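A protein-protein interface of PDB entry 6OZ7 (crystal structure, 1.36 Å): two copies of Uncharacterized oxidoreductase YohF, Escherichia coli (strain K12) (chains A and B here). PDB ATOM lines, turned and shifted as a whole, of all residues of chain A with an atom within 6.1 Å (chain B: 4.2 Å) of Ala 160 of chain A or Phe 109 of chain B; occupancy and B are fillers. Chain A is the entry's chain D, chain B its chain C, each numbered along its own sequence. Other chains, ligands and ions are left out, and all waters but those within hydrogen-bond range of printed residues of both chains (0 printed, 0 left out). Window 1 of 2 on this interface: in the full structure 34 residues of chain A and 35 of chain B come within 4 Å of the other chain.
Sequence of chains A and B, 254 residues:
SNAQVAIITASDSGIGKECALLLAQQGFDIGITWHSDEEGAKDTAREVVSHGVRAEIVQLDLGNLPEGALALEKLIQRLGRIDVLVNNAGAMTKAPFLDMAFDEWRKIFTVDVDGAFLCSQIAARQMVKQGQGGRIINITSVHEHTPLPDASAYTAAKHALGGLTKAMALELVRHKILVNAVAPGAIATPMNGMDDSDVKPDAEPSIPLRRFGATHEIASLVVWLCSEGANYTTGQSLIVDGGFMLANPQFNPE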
ATOM      1  N   ARG A 106       2.288  -0.248 -22.691  1.00  0.00           N
ATOM      2  CA  ARG A 106       1.679  -1.089 -21.639  1.00  0.00           C
ATOM      3  C   ARG A 106       0.283  -1.549 -22.070  1.00  0.00           C
ATOM      4  O   ARG A 106      -0.044  -2.715 -21.804  1.00  0.00           O
ATOM      5  CB  ARG A 106       1.631  -0.335 -20.318  1.00  0.00           C
ATOM      6  CG  ARG A 106       2.982  -0.383 -19.635  1.00  0.00           C
ATOM      7  CD  ARG A 106       2.984  -0.097 -18.164  1.00  0.00           C
ATOM      8  NE  ARG A 106       4.176  -0.664 -17.542  1.00  0.00           N
ATOM      9  CZ  ARG A 106       4.555  -0.403 -16.299  1.00  0.00           C
ATOM     10  NH1 ARG A 106       3.834   0.430 -15.561  1.00  0.00           N
ATOM     11  NH2 ARG A 106       5.644  -0.972 -15.805  1.00  0.00           N
ATOM     12  N   PHE A 109       0.399  -4.652 -24.249  1.00  0.00           N
ATOM     13  CA  PHE A 109       0.674  -5.869 -23.449  1.00  0.00           C
ATOM     14  C   PHE A 109      -0.580  -6.268 -22.657  1.00  0.00           C
ATOM     15  O   PHE A 109      -0.920  -7.458 -22.583  1.00  0.00           O
ATOM     16  CB  PHE A 109       1.888  -5.677 -22.548  1.00  0.00           C
ATOM     17  CG  PHE A 109       3.188  -5.919 -23.269  1.00  0.00           C
ATOM     18  CD1 PHE A 109       3.756  -4.957 -24.089  1.00  0.00           C
ATOM     19  CD2 PHE A 109       3.818  -7.147 -23.167  1.00  0.00           C
ATOM     20  CE1 PHE A 109       4.955  -5.196 -24.742  1.00  0.00           C
ATOM     21  CE2 PHE A 109       5.026  -7.382 -23.805  1.00  0.00           C
ATOM     22  CZ  PHE A 109       5.599  -6.403 -24.595  1.00  0.00           C
ATOM     23  N   VAL A 113      -1.447  -9.769 -24.200  1.00  0.00           N
ATOM     24  CA  VAL A 113      -0.913 -10.964 -23.489  1.00  0.00           C
ATOM     25  C   VAL A 113      -1.501 -11.055 -22.076  1.00  0.00           C
ATOM     26  O   VAL A 113      -1.743 -12.195 -21.691  1.00  0.00           O
ATOM     27  CB  VAL A 113       0.623 -11.088 -23.569  1.00  0.00           C
ATOM     28  CG1 VAL A 113       1.321 -10.021 -22.755  1.00  0.00           C
ATOM     29  CG2 VAL A 113       1.102 -12.481 -23.179  1.00  0.00           C
ATOM     30  N   ASP A 114      -1.738  -9.957 -21.356  1.00  0.00           N
ATOM     31  CA  ASP A 114      -2.225 -10.085 -19.958  1.00  0.00           C
ATOM     32  C   ASP A 114      -3.590 -10.788 -19.940  1.00  0.00           C
ATOM     33  O   ASP A 114      -3.832 -11.628 -19.046  1.00  0.00           O
ATOM     34  CB  ASP A 114      -2.279  -8.737 -19.251  1.00  0.00           C
ATOM     35  CG  ASP A 114      -0.928  -8.094 -18.998  1.00  0.00           C
ATOM     36  OD1 ASP A 114       0.114  -8.789 -19.140  1.00  0.00           O
ATOM     37  OD2 ASP A 114      -0.940  -6.919 -18.604  1.00  0.00           O
ATOM     38  N   THR A 155       4.594  -6.624 -31.912  1.00  0.00           N
ATOM     39  CA  THR A 155       5.560  -7.711 -32.170  1.00  0.00           C
ATOM     40  C   THR A 155       6.021  -8.310 -30.823  1.00  0.00           C
ATOM     41  O   THR A 155       6.083  -9.546 -30.646  1.00  0.00           O
ATOM     42  CB  THR A 155       6.755  -7.210 -32.994  1.00  0.00           C
ATOM     43  OG1 THR A 155       6.313  -6.727 -34.270  1.00  0.00           O
ATOM     44  CG2 THR A 155       7.759  -8.318 -33.205  1.00  0.00           C
ATOM     45  N   ALA A 156       6.436  -7.464 -29.902  1.00  0.00           N
ATOM     46  CA  ALA A 156       6.981  -7.907 -28.603  1.00  0.00           C
ATOM     47  C   ALA A 156       5.891  -8.675 -27.834  1.00  0.00           C
ATOM     48  O   ALA A 156       6.209  -9.717 -27.234  1.00  0.00           O
ATOM     49  CB  ALA A 156       7.549  -6.715 -27.835  1.00  0.00           C
ATOM     50  N   ALA A 157       4.640  -8.218 -27.869  1.00  0.00           N
ATOM     51  CA  ALA A 157       3.557  -8.898 -27.132  1.00  0.00           C
ATOM     52  C   ALA A 157       3.218 -10.242 -27.803  1.00  0.00           C
ATOM     53  O   ALA A 157       2.886 -11.215 -27.079  1.00  0.00           O
ATOM     54  CB  ALA A 157       2.372  -7.983 -26.989  1.00  0.00           C
ATOM     55  N   LYS A 158       3.232 -10.317 -29.129  1.00  0.00           N
ATOM     56  CA  LYS A 158       3.027 -11.621 -29.801  1.00  0.00           C
ATOM     57  C   LYS A 158       4.135 -12.592 -29.393  1.00  0.00           C
ATOM     58  O   LYS A 158       3.848 -13.767 -29.170  1.00  0.00           O
ATOM     59  CB  LYS A 158       2.934 -11.469 -31.324  1.00  0.00           C
ATOM     60  CG  LYS A 158       1.592 -10.865 -31.754  1.00  0.00           C
ATOM     61  CD  LYS A 158       0.400 -11.811 -31.563  1.00  0.00           C
ATOM     62  CE  LYS A 158      -0.933 -11.189 -31.944  1.00  0.00           C
ATOM     63  NZ  LYS A 158      -1.420 -10.265 -30.893  1.00  0.00           N
ATOM     64  N   HIS A 159       5.374 -12.125 -29.378  1.00  0.00           N
ATOM     65  CA  HIS A 159       6.483 -12.990 -28.918  1.00  0.00           C
ATOM     66  C   HIS A 159       6.225 -13.422 -27.472  1.00  0.00           C
ATOM     67  O   HIS A 159       6.437 -14.595 -27.164  1.00  0.00           O
ATOM     68  CB  HIS A 159       7.832 -12.288 -29.037  1.00  0.00           C
ATOM     69  CG  HIS A 159       8.451 -12.311 -30.396  1.00  0.00           C
ATOM     70  ND1 HIS A 159       7.911 -11.695 -31.517  1.00  0.00           N
ATOM     71  CD2 HIS A 159       9.645 -12.833 -30.775  1.00  0.00           C
ATOM     72  CE1 HIS A 159       8.751 -11.882 -32.532  1.00  0.00           C
ATOM     73  NE2 HIS A 159       9.801 -12.570 -32.107  1.00  0.00           N
ATOM     74  N   ALA A 160       5.784 -12.500 -26.613  1.00  0.00           N
ATOM     75  CA  ALA A 160       5.494 -12.843 -25.199  1.00  0.00           C
ATOM     76  C   ALA A 160       4.468 -13.974 -25.134  1.00  0.00           C
ATOM     77  O   ALA A 160       4.654 -14.918 -24.357  1.00  0.00           O
ATOM     78  CB  ALA A 160       4.959 -11.633 -24.454  1.00  0.00           C
ATOM     79  N   LEU A 161       3.416 -13.875 -25.940  1.00  0.00           N
ATOM     80  CA  LEU A 161       2.354 -14.895 -25.931  1.00  0.00           C
ATOM     81  C   LEU A 161       2.904 -16.210 -26.466  1.00  0.00           C
ATOM     82  O   LEU A 161       2.522 -17.266 -25.957  1.00  0.00           O
ATOM     83  CB  LEU A 161       1.123 -14.397 -26.672  1.00  0.00           C
ATOM     84  CG  LEU A 161      -0.108 -15.316 -26.609  1.00  0.00           C
ATOM     85  CD1 LEU A 161      -0.463 -15.791 -25.201  1.00  0.00           C
ATOM     86  CD2 LEU A 161      -1.299 -14.639 -27.292  1.00  0.00           C
ATOM     87  N   GLY A 162       3.835 -16.157 -27.414  1.00  0.00           N
ATOM     88  CA  GLY A 162       4.490 -17.386 -27.859  1.00  0.00           C
ATOM     89  C   GLY A 162       5.308 -18.029 -26.767  1.00  0.00           C
ATOM     90  O   GLY A 162       5.304 -19.282 -26.628  1.00  0.00           O
ATOM     91  N   GLY A 163       6.032 -17.227 -25.989  1.00  0.00           N
ATOM     92  CA  GLY A 163       6.804 -17.787 -24.862  1.00  0.00           C
ATOM     93  C   GLY A 163       5.886 -18.343 -23.790  1.00  0.00           C
ATOM     94  O   GLY A 163       6.167 -19.391 -23.235  1.00  0.00           O
ATOM     95  N   LEU A 164       4.819 -17.621 -23.483  1.00  0.00           N
ATOM     96  CA  LEU A 164       3.831 -18.133 -22.497  1.00  0.00           C
ATOM     97  C   LEU A 164       3.243 -19.470 -22.987  1.00  0.00           C
ATOM     98  O   LEU A 164       3.065 -20.379 -22.183  1.00  0.00           O
ATOM     99  CB  LEU A 164       2.719 -17.109 -22.281  1.00  0.00           C
ATOM    100  CG  LEU A 164       1.623 -17.558 -21.308  1.00  0.00           C
ATOM    101  CD1 LEU A 164       2.177 -17.844 -19.908  1.00  0.00           C
ATOM    102  CD2 LEU A 164       0.545 -16.515 -21.248  1.00  0.00           C
ATOM    103  N   THR A 165       2.981 -19.602 -24.276  1.00  0.00           N
ATOM    104  CA  THR A 165       2.498 -20.866 -24.864  1.00  0.00           C
ATOM    105  C   THR A 165       3.448 -22.013 -24.536  1.00  0.00           C
ATOM    106  O   THR A 165       2.997 -23.071 -24.080  1.00  0.00           O
ATOM    107  CB  THR A 165       2.254 -20.697 -26.355  1.00  0.00           C
ATOM    108  OG1 THR A 165       1.288 -19.671 -26.598  1.00  0.00           O
ATOM    109  CG2 THR A 165       1.823 -21.986 -27.002  1.00  0.00           C
ATOM    110  N   TRP B 105       3.270 -11.249 -12.085  1.00  0.00           N
ATOM    111  CA  TRP B 105       3.371 -11.341 -13.555  1.00  0.00           C
ATOM    112  C   TRP B 105       3.801  -9.974 -14.105  1.00  0.00           C
ATOM    113  O   TRP B 105       4.780  -9.893 -14.867  1.00  0.00           O
ATOM    114  CB  TRP B 105       2.033 -11.859 -14.115  1.00  0.00           C
ATOM    115  CG  TRP B 105       1.847 -11.681 -15.591  1.00  0.00           C
ATOM    116  CD1 TRP B 105       1.201 -10.663 -16.209  1.00  0.00           C
ATOM    117  CD2 TRP B 105       2.240 -12.584 -16.638  1.00  0.00           C
ATOM    118  NE1 TRP B 105       1.197 -10.839 -17.561  1.00  0.00           N
ATOM    119  CE2 TRP B 105       1.834 -12.012 -17.862  1.00  0.00           C
ATOM    120  CE3 TRP B 105       2.918 -13.803 -16.665  1.00  0.00           C
ATOM    121  CZ2 TRP B 105       2.046 -12.643 -19.090  1.00  0.00           C
ATOM    122  CZ3 TRP B 105       3.127 -14.425 -17.879  1.00  0.00           C
ATOM    123  CH2 TRP B 105       2.702 -13.854 -19.068  1.00  0.00           C
ATOM    124  N   ARG B 106       3.121  -8.909 -13.705  1.00  0.00           N
ATOM    125  CA  ARG B 106       3.394  -7.577 -14.287  1.00  0.00           C
ATOM    126  C   ARG B 106       4.765  -7.090 -13.817  1.00  0.00           C
ATOM    127  O   ARG B 106       5.440  -6.462 -14.600  1.00  0.00           O
ATOM    128  CB  ARG B 106       2.266  -6.610 -13.943  1.00  0.00           C
ATOM    129  CG  ARG B 106       1.071  -6.809 -14.856  1.00  0.00           C
ATOM    130  CD  ARG B 106       0.140  -5.641 -14.826  1.00  0.00           C
ATOM    131  NE  ARG B 106      -0.747  -5.633 -15.981  1.00  0.00           N
ATOM    132  CZ  ARG B 106      -1.785  -4.816 -16.105  1.00  0.00           C
ATOM    133  NH1 ARG B 106      -2.055  -3.947 -15.142  1.00  0.00           N
ATOM    134  NH2 ARG B 106      -2.542  -4.865 -17.185  1.00  0.00           N
ATOM    135  N   LYS B 107       5.167  -7.397 -12.593  1.00  0.00           N
ATOM    136  CA  LYS B 107       6.469  -6.915 -12.057  1.00  0.00           C
ATOM    137  C   LYS B 107       7.604  -7.507 -12.891  1.00  0.00           C
ATOM    138  O   LYS B 107       8.584  -6.795 -13.186  1.00  0.00           O
ATOM    139  CB  LYS B 107       6.648  -7.302 -10.588  1.00  0.00           C
ATOM    140  CG  LYS B 107       7.954  -6.816  -9.991  1.00  0.00           C
ATOM    141  CD  LYS B 107       8.053  -6.941  -8.502  1.00  0.00           C
ATOM    142  CE  LYS B 107       9.454  -6.624  -8.018  1.00  0.00           C
ATOM    143  NZ  LYS B 107       9.527  -6.564  -6.541  1.00  0.00           N
ATOM    144  N   ILE B 108       7.465  -8.765 -13.293  1.00  0.00           N
ATOM    145  CA  ILE B 108       8.509  -9.420 -14.113  1.00  0.00           C
ATOM    146  C   ILE B 108       8.569  -8.704 -15.467  1.00  0.00           C
ATOM    147  O   ILE B 108       9.678  -8.499 -15.971  1.00  0.00           O
ATOM    148  CB  ILE B 108       8.288 -10.947 -14.205  1.00  0.00           C
ATOM    149  CG1 ILE B 108       8.585 -11.581 -12.842  1.00  0.00           C
ATOM    150  CG2 ILE B 108       9.130 -11.576 -15.291  1.00  0.00           C
ATOM    151  CD1 ILE B 108       7.927 -12.895 -12.574  1.00  0.00           C
ATOM    152  N   PHE B 109       7.446  -8.394 -16.099  1.00  0.00           N
ATOM    153  CA  PHE B 109       7.478  -7.621 -17.358  1.00  0.00           C
ATOM    154  C   PHE B 109       8.059  -6.228 -17.129  1.00  0.00           C
ATOM    155  O   PHE B 109       8.839  -5.729 -17.984  1.00  0.00           O
ATOM    156  CB  PHE B 109       6.096  -7.551 -17.993  1.00  0.00           C
ATOM    157  CG  PHE B 109       5.777  -8.791 -18.783  1.00  0.00           C
ATOM    158  CD1 PHE B 109       5.345  -9.966 -18.166  1.00  0.00           C
ATOM    159  CD2 PHE B 109       5.978  -8.818 -20.150  1.00  0.00           C
ATOM    160  CE1 PHE B 109       5.062 -11.094 -18.915  1.00  0.00           C
ATOM    161  CE2 PHE B 109       5.662  -9.942 -20.899  1.00  0.00           C
ATOM    162  CZ  PHE B 109       5.247 -11.096 -20.280  1.00  0.00           C
ATOM    163  N   THR B 110       7.766  -5.585 -16.010  1.00  0.00           N
ATOM    164  CA  THR B 110       8.315  -4.241 -15.733  1.00  0.00           C
ATOM    165  C   THR B 110       9.841  -4.327 -15.743  1.00  0.00           C
ATOM    166  O   THR B 110      10.498  -3.500 -16.401  1.00  0.00           O
ATOM    167  CB  THR B 110       7.765  -3.710 -14.418  1.00  0.00           C
ATOM    168  OG1 THR B 110       6.350  -3.606 -14.548  1.00  0.00           O
ATOM    169  CG2 THR B 110       8.375  -2.390 -14.018  1.00  0.00           C
ATOM    170  N   VAL B 111      10.395  -5.243 -14.963  1.00  0.00           N
ATOM    171  CA  VAL B 111      11.859  -5.306 -14.709  1.00  0.00           C
ATOM    172  C   VAL B 111      12.550  -5.910 -15.940  1.00  0.00           C
ATOM    173  O   VAL B 111      13.648  -5.462 -16.294  1.00  0.00           O
ATOM    174  CB  VAL B 111      12.124  -6.065 -13.392  1.00  0.00           C
ATOM    175  CG1 VAL B 111      13.590  -6.210 -13.102  1.00  0.00           C
ATOM    176  CG2 VAL B 111      11.416  -5.388 -12.218  1.00  0.00           C
ATOM    177  N   ASP B 112      11.948  -6.879 -16.618  1.00  0.00           N
ATOM    178  CA  ASP B 112      12.660  -7.680 -17.653  1.00  0.00           C
ATOM    179  C   ASP B 112      12.358  -7.206 -19.089  1.00  0.00           C
ATOM    180  O   ASP B 112      13.072  -7.666 -19.997  1.00  0.00           O
ATOM    181  CB  ASP B 112      12.410  -9.176 -17.497  1.00  0.00           C
ATOM    182  CG  ASP B 112      13.017  -9.780 -16.236  1.00  0.00           C
ATOM    183  OD1 ASP B 112      13.880  -9.107 -15.568  1.00  0.00           O
ATOM    184  OD2 ASP B 112      12.628 -10.913 -15.909  1.00  0.00           O
ATOM    185  N   VAL B 113      11.357  -6.356 -19.342  1.00  0.00           N
ATOM    186  CA  VAL B 113      11.040  -5.833 -20.710  1.00  0.00           C
ATOM    187  C   VAL B 113      10.888  -4.313 -20.687  1.00  0.00           C
ATOM    188  O   VAL B 113      11.427  -3.636 -21.550  1.00  0.00           O
ATOM    189  CB  VAL B 113       9.743  -6.439 -21.276  1.00  0.00           C
ATOM    190  CG1 VAL B 113       9.672  -6.224 -22.774  1.00  0.00           C
ATOM    191  CG2 VAL B 113       9.622  -7.899 -20.915  1.00  0.00           C
ATOM    192  N   ASP B 114      10.074  -3.811 -19.770  1.00  0.00           N
ATOM    193  CA  ASP B 114       9.684  -2.378 -19.826  1.00  0.00           C
ATOM    194  C   ASP B 114      10.906  -1.483 -19.602  1.00  0.00           C
ATOM    195  O   ASP B 114      11.011  -0.449 -20.290  1.00  0.00           O
ATOM    196  CB  ASP B 114       8.601  -2.027 -18.798  1.00  0.00           C
ATOM    197  CG  ASP B 114       7.263  -2.660 -19.045  1.00  0.00           C
ATOM    198  OD1 ASP B 114       7.051  -3.204 -20.149  1.00  0.00           O
ATOM    199  OD2 ASP B 114       6.439  -2.588 -18.126  1.00  0.00           O
ATOM    200  N   ALA B 153       6.424 -16.430 -16.466  1.00  0.00           N
ATOM    201  CA  ALA B 153       6.519 -14.963 -16.636  1.00  0.00           C
ATOM    202  C   ALA B 153       7.920 -14.609 -17.167  1.00  0.00           C
ATOM    203  O   ALA B 153       8.016 -13.838 -18.131  1.00  0.00           O
ATOM    204  CB  ALA B 153       6.232 -14.266 -15.326  1.00  0.00           C
ATOM    205  N   ALA B 156       8.107 -15.713 -20.817  1.00  0.00           N
ATOM    206  CA  ALA B 156       7.308 -14.815 -21.663  1.00  0.00           C
ATOM    207  C   ALA B 156       8.001 -13.462 -21.840  1.00  0.00           C
ATOM    208  O   ALA B 156       8.008 -12.926 -22.974  1.00  0.00           O
ATOM    209  CB  ALA B 156       5.915 -14.684 -21.109  1.00  0.00           C
ATOM    210  N   ALA B 157       8.585 -12.939 -20.787  1.00  0.00           N
ATOM    211  CA  ALA B 157       9.226 -11.606 -20.826  1.00  0.00           C
ATOM    212  C   ALA B 157      10.530 -11.709 -21.639  1.00  0.00           C
ATOM    213  O   ALA B 157      10.835 -10.763 -22.360  1.00  0.00           O
ATOM    214  CB  ALA B 157       9.449 -11.040 -19.447  1.00  0.00           C
ATOM    215  N   ALA B 160       9.441 -11.656 -25.131  1.00  0.00           N
ATOM    216  CA  ALA B 160       9.032 -10.272 -25.451  1.00  0.00           C
ATOM    217  C   ALA B 160      10.272  -9.443 -25.819  1.00  0.00           C
ATOM    218  O   ALA B 160      10.224  -8.684 -26.814  1.00  0.00           O
ATOM    219  CB  ALA B 160       8.307  -9.635 -24.288  1.00  0.00           C
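NE1 of Trp 105 of chain B is in hydrogen-bond range of OD1 of Asp 114 of chain A. The guanidinium group (NE) of Arg 106 of chain B is in salt-bridge range of the side-chain carboxylate (OD2) of Asp 114 of chain A, 2.9 Å away. The side-chain hydroxyl (OG1) of Thr 110 of chain B sits at hydrogen-bond distance from the guanidinium group (NH2) of Arg 106 of chain A. The side-chain carboxylate of Asp 114 of chain B lies within salt-bridge range of the guanidinium group of Arg 106 of chain A, 2.9 Å away.
OG1 of Thr 110 of chain B is in hydrogen-bond range of O of Arg 106 of chain B, at 3.0 Å. The backbone carbonyl oxygen (O) of Phe 109 of chain B sits at hydrogen-bond distance from the backbone NH (N) of Asp 114 of chain B, 2.9 Å away. The backbone carbonyl oxygen of Phe 109 of chain A lies within hydrogen-bond range of the backbone NH of Asp 114 of chain A (2.9 Å).
Among the printed residues, pairs that only touch across the chains: Ala 160 of chain A with Ala 156 of chain B (3.4 Å), Ala 156 of chain A with Ala 160 of chain B (3.4 Å), Ala 160 of chain A with Ala 160 of chain B (3.9 Å), Phe 109 of chain A with Phe 109 of chain B (3.9 Å), Leu 164 of chain A with Ala 156 of chain B (3.9 Å) and Ala 160 of chain A with Phe 109 of chain B (3.999 Å).
Of the printed residues of chain B, Asp 114 of chain A touches Trp 105 (2.8 Å) and Arg 106 (2.9 Å). Printed residues of chain B within 4 Å of Ala 156 of chain A: Ala 160. Lys 158 of chain A touches none of the printed residues of chain B. Of the printed residues of chain B, Ala 160 of chain A touches Phe 109, Ala 156 and Ala 160. Of the printed residues of chain A, Trp 105 of chain B touches Asp 114 (2.8 Å). Printed residues of chain A within 4 Å of Phe 109 of chain B: Phe 109 (3.9 Å) and Ala 160 (3.999 Å). Val 111 of chain B touches none of the printed residues of chain A. Of the printed residues of chain A, Asp 114 of chain B touches Arg 106. The nearest printed residue of chain A that does not touch Phe 109 of chain B is Val 113 of chain A (4.7 Å). The nearest printed residue of chain A that does not touch Trp 105 of chain B is Leu 164 of chain A (4.1 Å).
Hydrophobic or aromatic side chains of chain A within 4 Å of the printed part of chain B: Phe 109, Ala 156 and Ala 160. Printed residues of chain B that touch a printed residue of chain A: Trp 105, Arg 106, Phe 109, Thr 110, Asp 114, Ala 156 and Ala 160. Hydrophobic or aromatic side chains of chain B within 4 Å of the printed part of chain A: Trp 105, Phe 109, Ala 156 and Ala 160. Among the printed residues, 10 pairs touch across the chains.
Arg 106 of chain A touches Asp 114 of chain B, and with the chains exchanged Asp 114 of chain A touches Arg 106 of chain B. Phe 109 of chain A touches its own counterpart, Phe 109 of chain B. Ala 156 of chain A touches Ala 160 of chain B, and with the chains exchanged Ala 160 of chain A touches Ala 156 of chain B. Ala 160 of chain A touches Phe 109 of chain B, but with the chains exchanged Phe 109 of chain A does not touch Ala 160 of chain B (4.01 Å). 7 positions are printed for both chains. Of the 10 pairs that touch across the chains among the printed residues, 6 have their exchanged pair printed and touching as well.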
